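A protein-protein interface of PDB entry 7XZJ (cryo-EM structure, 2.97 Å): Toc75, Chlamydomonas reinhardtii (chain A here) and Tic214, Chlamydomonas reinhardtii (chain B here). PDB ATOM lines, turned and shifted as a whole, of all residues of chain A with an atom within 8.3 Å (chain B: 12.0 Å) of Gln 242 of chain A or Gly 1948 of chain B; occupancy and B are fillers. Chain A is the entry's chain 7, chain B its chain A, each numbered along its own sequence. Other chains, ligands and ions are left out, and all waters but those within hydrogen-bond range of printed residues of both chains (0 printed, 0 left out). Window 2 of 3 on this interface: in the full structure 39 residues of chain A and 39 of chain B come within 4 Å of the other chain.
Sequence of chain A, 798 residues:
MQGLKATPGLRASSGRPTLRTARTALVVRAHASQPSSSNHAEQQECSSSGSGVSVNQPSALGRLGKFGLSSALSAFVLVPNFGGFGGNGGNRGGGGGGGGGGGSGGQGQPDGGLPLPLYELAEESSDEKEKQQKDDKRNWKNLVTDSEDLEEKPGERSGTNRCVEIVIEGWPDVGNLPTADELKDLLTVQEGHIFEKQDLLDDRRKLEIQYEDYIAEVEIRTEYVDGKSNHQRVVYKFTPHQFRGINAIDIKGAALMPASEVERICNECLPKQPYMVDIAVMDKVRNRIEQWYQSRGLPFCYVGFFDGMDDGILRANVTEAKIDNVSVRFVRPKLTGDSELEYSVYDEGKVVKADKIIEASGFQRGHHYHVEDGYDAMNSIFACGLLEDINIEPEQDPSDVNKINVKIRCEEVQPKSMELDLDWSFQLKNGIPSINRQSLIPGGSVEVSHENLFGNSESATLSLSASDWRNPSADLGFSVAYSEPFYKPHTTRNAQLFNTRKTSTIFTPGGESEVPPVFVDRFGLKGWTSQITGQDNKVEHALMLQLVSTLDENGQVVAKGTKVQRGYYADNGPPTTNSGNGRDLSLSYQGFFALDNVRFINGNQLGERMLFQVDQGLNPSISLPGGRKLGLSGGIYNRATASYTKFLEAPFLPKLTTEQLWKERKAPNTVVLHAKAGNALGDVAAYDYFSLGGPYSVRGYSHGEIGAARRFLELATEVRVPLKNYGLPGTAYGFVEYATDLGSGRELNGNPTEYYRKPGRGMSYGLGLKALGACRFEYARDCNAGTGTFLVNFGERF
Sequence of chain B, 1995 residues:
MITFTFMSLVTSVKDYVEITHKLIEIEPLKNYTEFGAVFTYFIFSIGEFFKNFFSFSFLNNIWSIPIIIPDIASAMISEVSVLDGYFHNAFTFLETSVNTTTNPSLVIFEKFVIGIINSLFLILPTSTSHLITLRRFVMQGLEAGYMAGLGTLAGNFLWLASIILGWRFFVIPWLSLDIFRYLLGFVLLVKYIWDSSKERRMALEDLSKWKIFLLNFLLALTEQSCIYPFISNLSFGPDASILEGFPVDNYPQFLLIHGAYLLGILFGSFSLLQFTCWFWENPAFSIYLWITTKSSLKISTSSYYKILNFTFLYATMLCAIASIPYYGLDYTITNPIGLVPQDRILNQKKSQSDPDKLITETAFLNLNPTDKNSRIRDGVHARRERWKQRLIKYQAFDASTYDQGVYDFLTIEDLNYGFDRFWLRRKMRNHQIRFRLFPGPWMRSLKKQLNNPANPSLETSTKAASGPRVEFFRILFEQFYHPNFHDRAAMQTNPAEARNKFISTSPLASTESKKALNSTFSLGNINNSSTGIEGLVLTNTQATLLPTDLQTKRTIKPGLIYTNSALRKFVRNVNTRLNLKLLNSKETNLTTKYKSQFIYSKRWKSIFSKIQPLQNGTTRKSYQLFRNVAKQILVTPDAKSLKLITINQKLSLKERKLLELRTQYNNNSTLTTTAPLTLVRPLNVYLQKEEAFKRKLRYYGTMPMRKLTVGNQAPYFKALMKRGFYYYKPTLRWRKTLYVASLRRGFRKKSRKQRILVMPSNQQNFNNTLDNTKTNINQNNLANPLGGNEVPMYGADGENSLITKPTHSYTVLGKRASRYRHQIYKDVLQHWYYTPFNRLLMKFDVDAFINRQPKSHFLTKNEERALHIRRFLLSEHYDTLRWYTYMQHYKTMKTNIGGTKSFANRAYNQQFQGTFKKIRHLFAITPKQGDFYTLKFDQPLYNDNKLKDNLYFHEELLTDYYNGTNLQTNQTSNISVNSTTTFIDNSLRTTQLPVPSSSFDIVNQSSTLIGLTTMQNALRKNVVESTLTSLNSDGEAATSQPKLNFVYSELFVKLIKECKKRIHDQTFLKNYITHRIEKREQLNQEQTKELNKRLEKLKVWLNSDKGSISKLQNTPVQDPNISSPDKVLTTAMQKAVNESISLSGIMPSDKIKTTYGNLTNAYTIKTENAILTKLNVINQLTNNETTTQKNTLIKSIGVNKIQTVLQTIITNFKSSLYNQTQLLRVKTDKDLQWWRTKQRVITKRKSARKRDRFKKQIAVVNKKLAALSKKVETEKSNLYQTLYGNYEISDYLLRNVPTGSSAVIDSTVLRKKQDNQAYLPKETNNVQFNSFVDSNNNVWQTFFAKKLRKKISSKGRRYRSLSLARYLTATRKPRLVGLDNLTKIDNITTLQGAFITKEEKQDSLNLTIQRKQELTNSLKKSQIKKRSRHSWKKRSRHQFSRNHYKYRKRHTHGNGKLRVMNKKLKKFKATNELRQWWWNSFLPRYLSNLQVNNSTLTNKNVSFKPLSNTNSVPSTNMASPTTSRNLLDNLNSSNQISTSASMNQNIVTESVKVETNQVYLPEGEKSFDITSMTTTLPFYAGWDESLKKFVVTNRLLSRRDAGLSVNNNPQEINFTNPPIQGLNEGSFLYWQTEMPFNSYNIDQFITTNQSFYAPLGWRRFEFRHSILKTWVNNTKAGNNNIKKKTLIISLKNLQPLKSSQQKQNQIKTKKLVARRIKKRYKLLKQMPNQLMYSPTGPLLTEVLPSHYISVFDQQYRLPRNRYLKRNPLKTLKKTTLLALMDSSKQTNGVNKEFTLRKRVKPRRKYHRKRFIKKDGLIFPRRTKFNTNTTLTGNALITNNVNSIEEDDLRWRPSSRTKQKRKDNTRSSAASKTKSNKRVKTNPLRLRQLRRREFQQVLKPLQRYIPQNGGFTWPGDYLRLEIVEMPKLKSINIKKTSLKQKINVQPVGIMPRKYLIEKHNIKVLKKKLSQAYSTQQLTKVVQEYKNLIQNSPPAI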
ATOM      1  N   ASP A 213      25.234  27.299   0.563  1.00  0.00           N
ATOM      2  CA  ASP A 213      25.785  25.967   0.200  1.00  0.00           C
ATOM      3  C   ASP A 213      25.184  24.896   1.112  1.00  0.00           C
ATOM      4  O   ASP A 213      24.470  24.017   0.594  1.00  0.00           O
ATOM      5  CB  ASP A 213      27.314  25.958   0.269  1.00  0.00           C
ATOM      6  CG  ASP A 213      27.865  26.477   1.585  1.00  0.00           C
ATOM      7  OD1 ASP A 213      27.077  27.036   2.370  1.00  0.00           O
ATOM      8  OD2 ASP A 213      29.079  26.314   1.814  1.00  0.00           O
ATOM      9  N   TYR A 214      25.469  24.956   2.416  1.00  0.00           N
ATOM     10  CA  TYR A 214      25.027  23.899   3.361  1.00  0.00           C
ATOM     11  C   TYR A 214      23.511  23.912   3.538  1.00  0.00           C
ATOM     12  O   TYR A 214      22.936  22.825   3.688  1.00  0.00           O
ATOM     13  CB  TYR A 214      25.674  24.115   4.730  1.00  0.00           C
ATOM     14  CG  TYR A 214      27.174  24.258   4.722  1.00  0.00           C
ATOM     15  CD1 TYR A 214      27.994  23.183   4.425  1.00  0.00           C
ATOM     16  CD2 TYR A 214      27.779  25.464   5.037  1.00  0.00           C
ATOM     17  CE1 TYR A 214      29.373  23.304   4.428  1.00  0.00           C
ATOM     18  CE2 TYR A 214      29.156  25.602   5.046  1.00  0.00           C
ATOM     19  CZ  TYR A 214      29.957  24.518   4.737  1.00  0.00           C
ATOM     20  OH  TYR A 214      31.316  24.646   4.741  1.00  0.00           O
ATOM     21  N   ILE A 215      22.889  25.093   3.528  1.00  0.00           N
ATOM     22  CA  ILE A 215      21.426  25.159   3.822  1.00  0.00           C
ATOM     23  C   ILE A 215      20.647  25.367   2.523  1.00  0.00           C
ATOM     24  O   ILE A 215      20.915  26.361   1.824  1.00  0.00           O
ATOM     25  CB  ILE A 215      21.129  26.260   4.857  1.00  0.00           C
ATOM     26  CG1 ILE A 215      22.081  26.179   6.052  1.00  0.00           C
ATOM     27  CG2 ILE A 215      19.674  26.214   5.292  1.00  0.00           C
ATOM     28  CD1 ILE A 215      21.915  27.303   7.036  1.00  0.00           C
ATOM     29  N   ALA A 216      19.707  24.466   2.231  1.00  0.00           N
ATOM     30  CA  ALA A 216      18.872  24.585   1.016  1.00  0.00           C
ATOM     31  C   ALA A 216      17.806  25.654   1.234  1.00  0.00           C
ATOM     32  O   ALA A 216      17.587  26.451   0.301  1.00  0.00           O
ATOM     33  CB  ALA A 216      18.218  23.263   0.709  1.00  0.00           C
ATOM     34  N   THR A 239      16.479  23.922   6.270  1.00  0.00           N
ATOM     35  CA  THR A 239      16.518  22.611   5.565  1.00  0.00           C
ATOM     36  C   THR A 239      17.905  22.433   4.943  1.00  0.00           C
ATOM     37  O   THR A 239      18.167  23.063   3.912  1.00  0.00           O
ATOM     38  CB  THR A 239      15.361  22.460   4.567  1.00  0.00           C
ATOM     39  OG1 THR A 239      15.611  23.262   3.413  1.00  0.00           O
ATOM     40  CG2 THR A 239      14.019  22.824   5.162  1.00  0.00           C
ATOM     41  N   PRO A 240      18.819  21.635   5.538  1.00  0.00           N
ATOM     42  CA  PRO A 240      20.172  21.511   5.003  1.00  0.00           C
ATOM     43  C   PRO A 240      20.140  20.833   3.627  1.00  0.00           C
ATOM     44  O   PRO A 240      19.406  19.875   3.465  1.00  0.00           O
ATOM     45  CB  PRO A 240      20.898  20.630   6.030  1.00  0.00           C
ATOM     46  CG  PRO A 240      19.793  19.881   6.747  1.00  0.00           C
ATOM     47  CD  PRO A 240      18.597  20.811   6.726  1.00  0.00           C
ATOM     48  N   HIS A 241      20.897  21.368   2.664  1.00  0.00           N
ATOM     49  CA  HIS A 241      20.949  20.757   1.309  1.00  0.00           C
ATOM     50  C   HIS A 241      21.723  19.442   1.387  1.00  0.00           C
ATOM     51  O   HIS A 241      22.956  19.496   1.526  1.00  0.00           O
ATOM     52  CB  HIS A 241      21.550  21.713   0.274  1.00  0.00           C
ATOM     53  CG  HIS A 241      21.203  21.325  -1.124  1.00  0.00           C
ATOM     54  ND1 HIS A 241      20.222  21.973  -1.848  1.00  0.00           N
ATOM     55  CD2 HIS A 241      21.675  20.343  -1.921  1.00  0.00           C
ATOM     56  CE1 HIS A 241      20.115  21.417  -3.037  1.00  0.00           C
ATOM     57  NE2 HIS A 241      20.995  20.411  -3.105  1.00  0.00           N
ATOM     58  N   GLN A 242      21.014  18.314   1.320  1.00  0.00           N
ATOM     59  CA  GLN A 242      21.668  16.983   1.394  1.00  0.00           C
ATOM     60  C   GLN A 242      21.339  16.215   0.109  1.00  0.00           C
ATOM     61  O   GLN A 242      20.149  16.167  -0.254  1.00  0.00           O
ATOM     62  CB  GLN A 242      21.212  16.279   2.673  1.00  0.00           C
ATOM     63  CG  GLN A 242      19.718  16.401   2.939  1.00  0.00           C
ATOM     64  CD  GLN A 242      19.313  15.757   4.241  1.00  0.00           C
ATOM     65  OE1 GLN A 242      20.146  15.438   5.086  1.00  0.00           O
ATOM     66  NE2 GLN A 242      18.016  15.564   4.417  1.00  0.00           N
ATOM     67  N   PHE A 243      22.351  15.655  -0.562  1.00  0.00           N
ATOM     68  CA  PHE A 243      22.111  14.992  -1.872  1.00  0.00           C
ATOM     69  C   PHE A 243      22.864  13.660  -1.938  1.00  0.00           C
ATOM     70  O   PHE A 243      24.092  13.723  -2.163  1.00  0.00           O
ATOM     71  CB  PHE A 243      22.524  15.933  -3.008  1.00  0.00           C
ATOM     72  CG  PHE A 243      22.028  15.556  -4.380  1.00  0.00           C
ATOM     73  CD1 PHE A 243      20.785  15.975  -4.823  1.00  0.00           C
ATOM     74  CD2 PHE A 243      22.809  14.799  -5.238  1.00  0.00           C
ATOM     75  CE1 PHE A 243      20.329  15.636  -6.087  1.00  0.00           C
ATOM     76  CE2 PHE A 243      22.354  14.461  -6.502  1.00  0.00           C
ATOM     77  CZ  PHE A 243      21.114  14.880  -6.925  1.00  0.00           C
ATOM     78  N   ARG A 244      22.184  12.534  -1.676  1.00  0.00           N
ATOM     79  CA  ARG A 244      22.778  11.165  -1.770  1.00  0.00           C
ATOM     80  C   ARG A 244      23.502  10.811  -0.466  1.00  0.00           C
ATOM     81  O   ARG A 244      23.953  11.742   0.225  1.00  0.00           O
ATOM     82  CB  ARG A 244      23.626  10.960  -3.033  1.00  0.00           C
ATOM     83  N   GLY A 245      23.675   9.517  -0.182  1.00  0.00           N
ATOM     84  CA  GLY A 245      24.294   9.102   1.093  1.00  0.00           C
ATOM     85  C   GLY A 245      25.632   8.415   0.887  1.00  0.00           C
ATOM     86  O   GLY A 245      25.697   7.486   0.060  1.00  0.00           O
ATOM     87  N   TYR A 275      22.623   6.738   6.589  1.00  0.00           N
ATOM     88  CA  TYR A 275      21.327   6.801   5.859  1.00  0.00           C
ATOM     89  C   TYR A 275      21.044   8.242   5.423  1.00  0.00           C
ATOM     90  O   TYR A 275      21.966   9.077   5.528  1.00  0.00           O
ATOM     91  CB  TYR A 275      20.178   6.272   6.722  1.00  0.00           C
ATOM     92  CG  TYR A 275      20.052   4.770   6.759  1.00  0.00           C
ATOM     93  CD1 TYR A 275      19.588   4.066   5.661  1.00  0.00           C
ATOM     94  CD2 TYR A 275      20.399   4.050   7.890  1.00  0.00           C
ATOM     95  CE1 TYR A 275      19.473   2.686   5.684  1.00  0.00           C
ATOM     96  CE2 TYR A 275      20.291   2.671   7.930  1.00  0.00           C
ATOM     97  CZ  TYR A 275      19.824   1.986   6.824  1.00  0.00           C
ATOM     98  OH  TYR A 275      19.713   0.626   6.855  1.00  0.00           O
ATOM     99  N   MET A 276      19.829   8.517   4.936  1.00  0.00           N
ATOM    100  CA  MET A 276      19.453   9.882   4.468  1.00  0.00           C
ATOM    101  C   MET A 276      20.478  10.384   3.444  1.00  0.00           C
ATOM    102  O   MET A 276      20.857   9.595   2.554  1.00  0.00           O
ATOM    103  CB  MET A 276      19.360  10.873   5.632  1.00  0.00           C
ATOM    104  N   VAL A 277      20.938  11.632   3.577  1.00  0.00           N
ATOM    105  CA  VAL A 277      21.864  12.204   2.551  1.00  0.00           C
ATOM    106  C   VAL A 277      22.920  13.086   3.227  1.00  0.00           C
ATOM    107  O   VAL A 277      22.579  13.750   4.224  1.00  0.00           O
ATOM    108  CB  VAL A 277      21.076  12.972   1.474  1.00  0.00           C
ATOM    109  N   ASP A 278      24.151  13.111   2.696  1.00  0.00           N
ATOM    110  CA  ASP A 278      25.257  13.867   3.350  1.00  0.00           C
ATOM    111  C   ASP A 278      26.039  14.694   2.321  1.00  0.00           C
ATOM    112  O   ASP A 278      26.756  14.078   1.508  1.00  0.00           O
ATOM    113  CB  ASP A 278      26.237  12.913   4.037  1.00  0.00           C
ATOM    114  CG  ASP A 278      25.577  11.874   4.927  1.00  0.00           C
ATOM    115  OD1 ASP A 278      24.807  12.273   5.823  1.00  0.00           O
ATOM    116  OD2 ASP A 278      25.835  10.673   4.711  1.00  0.00           O
ATOM    117  N   ILE A 279      25.912  16.026   2.351  1.00  0.00           N
ATOM    118  CA  ILE A 279      26.721  16.899   1.443  1.00  0.00           C
ATOM    119  C   ILE A 279      27.710  17.727   2.278  1.00  0.00           C
ATOM    120  O   ILE A 279      28.791  18.065   1.747  1.00  0.00           O
ATOM    121  CB  ILE A 279      25.793  17.767   0.563  1.00  0.00           C
ATOM    122  CG1 ILE A 279      25.626  17.172  -0.837  1.00  0.00           C
ATOM    123  CG2 ILE A 279      26.248  19.217   0.503  1.00  0.00           C
ATOM    124  N   ALA A 280      27.395  17.974   3.554  1.00  0.00           N
ATOM    125  CA  ALA A 280      28.252  18.813   4.431  1.00  0.00           C
ATOM    126  C   ALA A 280      29.626  18.170   4.644  1.00  0.00           C
ATOM    127  O   ALA A 280      30.622  18.920   4.689  1.00  0.00           O
ATOM    128  CB  ALA A 280      27.553  19.058   5.745  1.00  0.00           C
ATOM    129  N   LEU B1723      26.858  27.847  -8.061  1.00  0.00           N
ATOM    130  CA  LEU B1723      25.767  26.885  -7.971  1.00  0.00           C
ATOM    131  C   LEU B1723      25.649  26.069  -9.253  1.00  0.00           C
ATOM    132  O   LEU B1723      25.474  24.847  -9.207  1.00  0.00           O
ATOM    133  CB  LEU B1723      24.456  27.612  -7.678  1.00  0.00           C
ATOM    134  CG  LEU B1723      23.178  26.773  -7.715  1.00  0.00           C
ATOM    135  CD1 LEU B1723      23.080  25.904  -6.474  1.00  0.00           C
ATOM    136  CD2 LEU B1723      21.946  27.655  -7.865  1.00  0.00           C
ATOM    137  N   GLN B1726      28.586  23.093 -10.008  1.00  0.00           N
ATOM    138  CA  GLN B1726      28.495  21.806  -9.334  1.00  0.00           C
ATOM    139  C   GLN B1726      27.157  21.106  -9.547  1.00  0.00           C
ATOM    140  O   GLN B1726      26.932  20.057  -8.938  1.00  0.00           O
ATOM    141  CB  GLN B1726      28.756  21.990  -7.837  1.00  0.00           C
ATOM    142  CG  GLN B1726      30.171  22.430  -7.504  1.00  0.00           C
ATOM    143  CD  GLN B1726      31.215  21.438  -7.974  1.00  0.00           C
ATOM    144  OE1 GLN B1726      31.025  20.227  -7.870  1.00  0.00           O
ATOM    145  NE2 GLN B1726      32.327  21.946  -8.494  1.00  0.00           N
ATOM    146  N   MET B1727      26.288  21.647 -10.404  1.00  0.00           N
ATOM    147  CA  MET B1727      24.936  21.108 -10.556  1.00  0.00           C
ATOM    148  C   MET B1727      24.890  19.623 -10.894  1.00  0.00           C
ATOM    149  O   MET B1727      24.063  18.909 -10.303  1.00  0.00           O
ATOM    150  CB  MET B1727      24.171  21.920 -11.605  1.00  0.00           C
ATOM    151  N   PRO B1728      25.695  19.095 -11.825  1.00  0.00           N
ATOM    152  CA  PRO B1728      25.571  17.658 -12.137  1.00  0.00           C
ATOM    153  C   PRO B1728      25.873  16.754 -10.954  1.00  0.00           C
ATOM    154  O   PRO B1728      25.118  15.808 -10.690  1.00  0.00           O
ATOM    155  CB  PRO B1728      26.576  17.466 -13.281  1.00  0.00           C
ATOM    156  CG  PRO B1728      27.533  18.587 -13.141  1.00  0.00           C
ATOM    157  CD  PRO B1728      26.707  19.740 -12.682  1.00  0.00           C
ATOM    158  N   ASN B1729      26.984  17.032 -10.267  1.00  0.00           N
ATOM    159  CA  ASN B1729      27.396  16.200  -9.108  1.00  0.00           C
ATOM    160  C   ASN B1729      26.421  16.424  -7.949  1.00  0.00           C
ATOM    161  O   ASN B1729      25.918  15.422  -7.406  1.00  0.00           O
ATOM    162  CB  ASN B1729      28.836  16.503  -8.687  1.00  0.00           C
ATOM    163  CG  ASN B1729      29.102  17.986  -8.539  1.00  0.00           C
ATOM    164  OD1 ASN B1729      29.076  18.520  -7.432  1.00  0.00           O
ATOM    165  ND2 ASN B1729      29.351  18.660  -9.650  1.00  0.00           N
ATOM    166  N   GLN B1730      26.165  17.686  -7.590  1.00  0.00           N
ATOM    167  CA  GLN B1730      25.285  17.984  -6.430  1.00  0.00           C
ATOM    168  C   GLN B1730      24.378  19.176  -6.744  1.00  0.00           C
ATOM    169  O   GLN B1730      24.766  20.002  -7.589  1.00  0.00           O
ATOM    170  CB  GLN B1730      26.134  18.309  -5.200  1.00  0.00           C
ATOM    171  CG  GLN B1730      27.381  17.449  -5.065  1.00  0.00           C
ATOM    172  CD  GLN B1730      27.054  15.996  -4.824  1.00  0.00           C
ATOM    173  OE1 GLN B1730      27.853  15.107  -5.107  1.00  0.00           O
ATOM    174  NE2 GLN B1730      25.863  15.743  -4.306  1.00  0.00           N
ATOM    175  N   LEU B1731      23.207  19.253  -6.106  1.00  0.00           N
ATOM    176  CA  LEU B1731      22.331  20.441  -6.274  1.00  0.00           C
ATOM    177  C   LEU B1731      22.030  20.723  -7.744  1.00  0.00           C
ATOM    178  O   LEU B1731      22.391  21.817  -8.213  1.00  0.00           O
ATOM    179  CB  LEU B1731      23.030  21.645  -5.632  1.00  0.00           C
ATOM    180  N   MET B1732      21.410  19.779  -8.451  1.00  0.00           N
ATOM    181  CA  MET B1732      20.971  20.089  -9.803  1.00  0.00           C
ATOM    182  C   MET B1732      19.884  21.155  -9.766  1.00  0.00           C
ATOM    183  O   MET B1732      18.954  21.085  -8.958  1.00  0.00           O
ATOM    184  CB  MET B1732      20.456  18.828 -10.498  1.00  0.00           C
ATOM    185  N   TYR B1733      20.013  22.148 -10.643  1.00  0.00           N
ATOM    186  CA  TYR B1733      19.105  23.293 -10.689  1.00  0.00           C
ATOM    187  C   TYR B1733      19.051  24.011  -9.347  1.00  0.00           C
ATOM    188  O   TYR B1733      19.958  24.763  -8.994  1.00  0.00           O
ATOM    189  CB  TYR B1733      17.697  22.858 -11.106  1.00  0.00           C
ATOM    190  N   GLY B1948      18.201  16.477  -2.512  1.00  0.00           N
ATOM    191  CA  GLY B1948      18.322  17.931  -2.739  1.00  0.00           C
ATOM    192  C   GLY B1948      17.060  18.510  -3.352  1.00  0.00           C
ATOM    193  O   GLY B1948      16.686  18.068  -4.456  1.00  0.00           O
ATOM    194  N   ILE B1949      16.424  19.464  -2.665  1.00  0.00           N
ATOM    195  CA  ILE B1949      15.147  20.059  -3.162  1.00  0.00           C
ATOM    196  C   ILE B1949      15.421  21.474  -3.676  1.00  0.00           C
ATOM    197  O   ILE B1949      16.440  22.064  -3.262  1.00  0.00           O
ATOM    198  CB  ILE B1949      14.077  20.059  -2.051  1.00  0.00           C
ATOM    199  CG1 ILE B1949      14.501  20.914  -0.854  1.00  0.00           C
ATOM    200  CG2 ILE B1949      13.733  18.638  -1.634  1.00  0.00           C
ATOM    201  CD1 ILE B1949      13.464  20.996   0.241  1.00  0.00           C
ATOM    202  N   MET B1950      14.554  21.990  -4.553  1.00  0.00           N
ATOM    203  CA  MET B1950      14.700  23.355  -5.036  1.00  0.00           C
ATOM    204  C   MET B1950      13.348  24.052  -4.951  1.00  0.00           C
ATOM    205  O   MET B1950      12.483  23.824  -5.810  1.00  0.00           O
ATOM    206  CB  MET B1950      15.229  23.369  -6.474  1.00  0.00           C
ATOM    207  CG  MET B1950      15.609  24.750  -6.976  1.00  0.00           C
ATOM    208  N   PRO B1951      13.065  24.907  -3.929  1.00  0.00           N
ATOM    209  CA  PRO B1951      11.718  25.480  -3.769  1.00  0.00           C
ATOM    210  C   PRO B1951      11.337  26.656  -4.678  1.00  0.00           C
ATOM    211  O   PRO B1951      12.062  27.635  -4.710  1.00  0.00           O
ATOM    212  CB  PRO B1951      11.674  25.907  -2.293  1.00  0.00           C
ATOM    213  CG  PRO B1951      13.102  26.278  -1.968  1.00  0.00           C
ATOM    214  CD  PRO B1951      13.961  25.400  -2.855  1.00  0.00           C
ATOM    215  N   ARG B1952      10.215  26.535  -5.394  1.00  0.00           N
ATOM    216  CA  ARG B1952       9.710  27.655  -6.232  1.00  0.00           C
ATOM    217  C   ARG B1952       8.314  27.999  -5.705  1.00  0.00           C
ATOM    218  O   ARG B1952       7.503  27.066  -5.565  1.00  0.00           O
ATOM    219  CB  ARG B1952       9.633  27.233  -7.703  1.00  0.00           C
ATOM    220  CG  ARG B1952      10.786  26.358  -8.175  1.00  0.00           C
ATOM    221  CD  ARG B1952      12.118  27.081  -8.247  1.00  0.00           C
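Of the 17 printed residues of chain A, 4 touch a printed residue of chain B.
Hydrophobic or aromatic side chains of chain A that line the printed part of chain B: His 241, Phe 243 and Ile 279.
Hydrophobic or aromatic side chains of chain B within 4 Å of the printed part of chain A: Leu 1731.
Along chain B the printed residues that touch a printed residue of chain A span positions 1729 to 1949.
Among the printed residues, 8 pairs touch across the chains.
Among the printed residues, no Asp or Glu carboxylate lies within 4 Å of a Lys or Arg side-chain nitrogen of the other chain.
The backbone carbonyl oxygen (O) of Gln 242 of chain A sits at hydrogen-bond distance from the backbone NH (N) of Gly 1948 of chain B.
O of Phe 243 of chain A sits close to NE2 of Gln 1730 of chain B (3.4 Å).
Among the printed residues, merely in contact across the chains: His 241 of chain A with Leu 1731 of chain B, Phe 243 of chain A with Gly 1948 of chain B, His 241 of chain A with Gly 1948 of chain B, His 241 of chain A with Ile 1949 of chain B, Ile 279 of chain A with Gln 1730 of chain B and Phe 243 of chain A with Asn 1729 of chain B.
Gln 242 of chain A touches just one residue of chain B: Gly 1948 (3.0 Å).
Gly 1948 of chain B touches three residues of chain A.
Of chain B, only Leu 1731 (3.4 Å), Gly 1948 (3.7 Å) and Ile 1949 (3.7 Å) come within 4 Å of His 241 of chain A.
No residue of chain B comes within 4 Å of Arg 244 of chain A.
No residue of chain B comes within 4 Å of Met 276 of chain A.
No residue of chain B comes within 4 Å of Val 277 of chain A.
No residue of chain B comes within 4 Å of Asp 278 of chain A.
Of chain B, only Gln 1730 comes within 4 Å of Ile 279 of chain A.
Printed residues of chain A within 4 Å of Gln 1730 of chain B: Phe 243 and Ile 279.
Of the printed residues of chain A, Asn 1729 of chain B touches Phe 243.
Printed residues of chain A within 4 Å of Ile 1949 of chain B: His 241 (3.7 Å).
Of the printed residues of chain A, Leu 1731 of chain B touches His 241.
Met 1950 of chain B touches none of the printed residues of chain A.
Met 1727 of chain B touches none of the printed residues of chain A.
The nearest residue of chain A that does not touch Gly 1948 of chain B is Arg 244 of chain A (5.7 Å).
The side-chain amide oxygen of Gln 1726 of chain B lies close to the side-chain amide oxygen of Asn 1729 of chain B (2.6 Å).
O of Tyr 214 of chain A sits at hydrogen-bond distance from N of His 241 of chain A, 2.7 Å away.
The side-chain amide oxygen of Gln 242 of chain A sits close to the backbone carbonyl oxygen of Val 277 of chain A (3.1 Å).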
